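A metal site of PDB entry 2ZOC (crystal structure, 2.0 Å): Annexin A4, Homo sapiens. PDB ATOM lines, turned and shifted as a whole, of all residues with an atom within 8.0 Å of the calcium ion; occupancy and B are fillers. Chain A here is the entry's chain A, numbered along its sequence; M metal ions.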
ATOM      1  N   ARG A  96     -10.758 -16.275 -32.804  1.00  0.00           N
ATOM      2  CA  ARG A  96     -11.014 -15.988 -31.395  1.00  0.00           C
ATOM      3  C   ARG A  96     -11.469 -17.258 -30.673  1.00  0.00           C
ATOM      4  O   ARG A  96     -10.940 -17.606 -29.614  1.00  0.00           O
ATOM      5  CB  ARG A  96     -12.101 -14.910 -31.273  1.00  0.00           C
ATOM      6  CG  ARG A  96     -12.547 -14.645 -29.850  1.00  0.00           C
ATOM      7  CD  ARG A  96     -11.472 -14.002 -28.989  1.00  0.00           C
ATOM      8  NE  ARG A  96     -12.058 -13.443 -27.775  1.00  0.00           N
ATOM      9  CZ  ARG A  96     -11.421 -12.705 -26.879  1.00  0.00           C
ATOM     10  NH1 ARG A  96     -10.129 -12.417 -27.046  1.00  0.00           N
ATOM     11  NH2 ARG A  96     -12.067 -12.224 -25.829  1.00  0.00           N
ATOM     12  N   ARG A  97     -12.441 -17.947 -31.262  1.00  0.00           N
ATOM     13  CA  ARG A  97     -12.955 -19.180 -30.683  1.00  0.00           C
ATOM     14  C   ARG A  97     -11.867 -20.230 -30.586  1.00  0.00           C
ATOM     15  O   ARG A  97     -11.821 -21.000 -29.629  1.00  0.00           O
ATOM     16  CB  ARG A  97     -14.131 -19.716 -31.511  1.00  0.00           C
ATOM     17  CG  ARG A  97     -15.012 -20.707 -30.771  1.00  0.00           C
ATOM     18  CD  ARG A  97     -16.451 -20.625 -31.261  1.00  0.00           C
ATOM     19  NE  ARG A  97     -16.626 -21.083 -32.632  1.00  0.00           N
ATOM     20  CZ  ARG A  97     -16.580 -22.355 -33.006  1.00  0.00           C
ATOM     21  NH1 ARG A  97     -16.373 -23.300 -32.110  1.00  0.00           N
ATOM     22  NH2 ARG A  97     -16.771 -22.684 -34.280  1.00  0.00           N
ATOM     23  N   ALA A  98     -10.979 -20.254 -31.571  1.00  0.00           N
ATOM     24  CA  ALA A  98      -9.879 -21.217 -31.565  1.00  0.00           C
ATOM     25  C   ALA A  98      -8.952 -21.018 -30.378  1.00  0.00           C
ATOM     26  O   ALA A  98      -8.344 -21.968 -29.895  1.00  0.00           O
ATOM     27  CB  ALA A  98      -9.082 -21.104 -32.860  1.00  0.00           C
ATOM     28  N   MET A  99      -8.844 -19.791 -29.886  1.00  0.00           N
ATOM     29  CA  MET A  99      -7.950 -19.505 -28.761  1.00  0.00           C
ATOM     30  C   MET A  99      -8.607 -19.326 -27.399  1.00  0.00           C
ATOM     31  O   MET A  99      -8.009 -19.625 -26.367  1.00  0.00           O
ATOM     32  CB  MET A  99      -7.108 -18.271 -29.078  1.00  0.00           C
ATOM     33  CG  MET A  99      -6.106 -18.479 -30.201  1.00  0.00           C
ATOM     34  SD  MET A  99      -5.127 -17.009 -30.536  1.00  0.00           S
ATOM     35  CE  MET A  99      -6.168 -16.193 -31.752  1.00  0.00           C
ATOM     36  N   LYS A 100      -9.843 -18.819 -27.382  1.00  0.00           N
ATOM     37  CA  LYS A 100     -10.522 -18.569 -26.112  1.00  0.00           C
ATOM     38  C   LYS A 100     -10.833 -19.826 -25.316  1.00  0.00           C
ATOM     39  O   LYS A 100     -11.358 -20.810 -25.848  1.00  0.00           O
ATOM     40  CB  LYS A 100     -11.814 -17.787 -26.355  1.00  0.00           C
ATOM     41  CG  LYS A 100     -12.478 -17.237 -25.081  1.00  0.00           C
ATOM     42  CD  LYS A 100     -13.590 -16.255 -25.433  1.00  0.00           C
ATOM     43  CE  LYS A 100     -14.142 -15.548 -24.188  1.00  0.00           C
ATOM     44  NZ  LYS A 100     -14.810 -16.477 -23.238  1.00  0.00           N
ATOM     45  N   GLY A 101     -10.490 -19.794 -24.031  1.00  0.00           N
ATOM     46  CA  GLY A 101     -10.744 -20.935 -23.163  1.00  0.00           C
ATOM     47  C   GLY A 101      -9.555 -21.873 -23.077  1.00  0.00           C
ATOM     48  O   GLY A 101      -8.517 -21.629 -23.702  1.00  0.00           O
ATOM     49  N   ALA A 102      -9.709 -22.944 -22.309  1.00  0.00           N
ATOM     50  CA  ALA A 102      -8.642 -23.931 -22.144  1.00  0.00           C
ATOM     51  C   ALA A 102      -8.158 -24.438 -23.498  1.00  0.00           C
ATOM     52  O   ALA A 102      -8.931 -24.593 -24.437  1.00  0.00           O
ATOM     53  CB  ALA A 102      -9.144 -25.109 -21.311  1.00  0.00           C
ATOM     54  N   GLY A 103      -6.849 -24.678 -23.581  1.00  0.00           N
ATOM     55  CA  GLY A 103      -6.264 -25.174 -24.806  1.00  0.00           C
ATOM     56  C   GLY A 103      -6.486 -24.301 -26.031  1.00  0.00           C
ATOM     57  O   GLY A 103      -6.899 -23.135 -25.927  1.00  0.00           O
ATOM     58  N   THR A 104      -6.198 -24.855 -27.201  1.00  0.00           N
ATOM     59  CA  THR A 104      -6.356 -24.112 -28.427  1.00  0.00           C
ATOM     60  C   THR A 104      -6.651 -25.041 -29.601  1.00  0.00           C
ATOM     61  O   THR A 104      -6.186 -26.180 -29.640  1.00  0.00           O
ATOM     62  CB  THR A 104      -5.095 -23.240 -28.739  1.00  0.00           C
ATOM     63  OG1 THR A 104      -4.721 -23.370 -30.111  1.00  0.00           O
ATOM     64  CG2 THR A 104      -3.938 -23.637 -27.854  1.00  0.00           C
ATOM     65  N   ASP A 105      -7.473 -24.558 -30.520  1.00  0.00           N
ATOM     66  CA  ASP A 105      -7.830 -25.311 -31.715  1.00  0.00           C
ATOM     67  C   ASP A 105      -6.723 -24.978 -32.708  1.00  0.00           C
ATOM     68  O   ASP A 105      -6.866 -24.050 -33.497  1.00  0.00           O
ATOM     69  CB  ASP A 105      -9.186 -24.848 -32.247  1.00  0.00           C
ATOM     70  CG  ASP A 105      -9.648 -25.630 -33.457  1.00  0.00           C
ATOM     71  OD1 ASP A 105      -8.796 -26.304 -34.092  1.00  0.00           O
ATOM     72  OD2 ASP A 105     -10.847 -25.565 -33.797  1.00  0.00           O
ATOM     73  N   ASP A 139      -3.099 -12.172 -28.742  1.00  0.00           N
ATOM     74  CA  ASP A 139      -3.766 -13.413 -28.350  1.00  0.00           C
ATOM     75  C   ASP A 139      -2.998 -14.654 -28.794  1.00  0.00           C
ATOM     76  O   ASP A 139      -2.977 -15.663 -28.097  1.00  0.00           O
ATOM     77  CB  ASP A 139      -5.201 -13.459 -28.879  1.00  0.00           C
ATOM     78  CG  ASP A 139      -6.178 -12.690 -27.991  1.00  0.00           C
ATOM     79  OD1 ASP A 139      -7.388 -12.719 -28.269  1.00  0.00           O
ATOM     80  OD2 ASP A 139      -5.723 -12.056 -27.014  1.00  0.00           O
ATOM     81  N   SER A 142      -0.346 -15.279 -26.400  1.00  0.00           N
ATOM     82  CA  SER A 142      -0.856 -15.749 -25.120  1.00  0.00           C
ATOM     83  C   SER A 142      -1.327 -17.197 -25.157  1.00  0.00           C
ATOM     84  O   SER A 142      -1.275 -17.904 -24.146  1.00  0.00           O
ATOM     85  CB  SER A 142      -2.001 -14.837 -24.673  1.00  0.00           C
ATOM     86  OG  SER A 142      -2.562 -15.304 -23.452  1.00  0.00           O
ATOM     87  N   ASP A 143      -1.791 -17.650 -26.316  1.00  0.00           N
ATOM     88  CA  ASP A 143      -2.299 -19.020 -26.461  1.00  0.00           C
ATOM     89  C   ASP A 143      -1.320 -20.050 -27.006  1.00  0.00           C
ATOM     90  O   ASP A 143      -1.547 -21.252 -26.868  1.00  0.00           O
ATOM     91  CB  ASP A 143      -3.546 -19.018 -27.341  1.00  0.00           C
ATOM     92  CG  ASP A 143      -4.721 -19.711 -26.690  1.00  0.00           C
ATOM     93  OD1 ASP A 143      -5.175 -19.219 -25.634  1.00  0.00           O
ATOM     94  OD2 ASP A 143      -5.184 -20.743 -27.223  1.00  0.00           O
ATOM     95  N   THR A 144      -0.237 -19.587 -27.639  1.00  0.00           N
ATOM     96  CA  THR A 144       0.726 -20.516 -28.204  1.00  0.00           C
ATOM     97  C   THR A 144       2.155 -20.194 -27.759  1.00  0.00           C
ATOM     98  O   THR A 144       2.426 -19.119 -27.223  1.00  0.00           O
ATOM     99  CB  THR A 144       0.675 -20.522 -29.756  1.00  0.00           C
ATOM    100  OG1 THR A 144       1.037 -19.223 -30.263  1.00  0.00           O
ATOM    101  CG2 THR A 144      -0.733 -20.861 -30.227  1.00  0.00           C
HETATM  102 CA    CA M   1      -6.692 -20.869 -25.125  1.00  0.00          CA
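Of the 14 residues printed, 4 come within 4 Å of the calcium ion.
The nearest printed residue that does not touch the calcium ion is Ala 102 (4.2 Å).
The calcium ion is bound by O of Met 99 (2.2 Å), OD1 of Asp 143 (2.3 Å), O of Gly 103 (2.4 Å), O of Gly 101 (2.4 Å) and OD2 of Asp 143 (2.6 Å).
The calcium ion has five donor atoms within binding distance.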
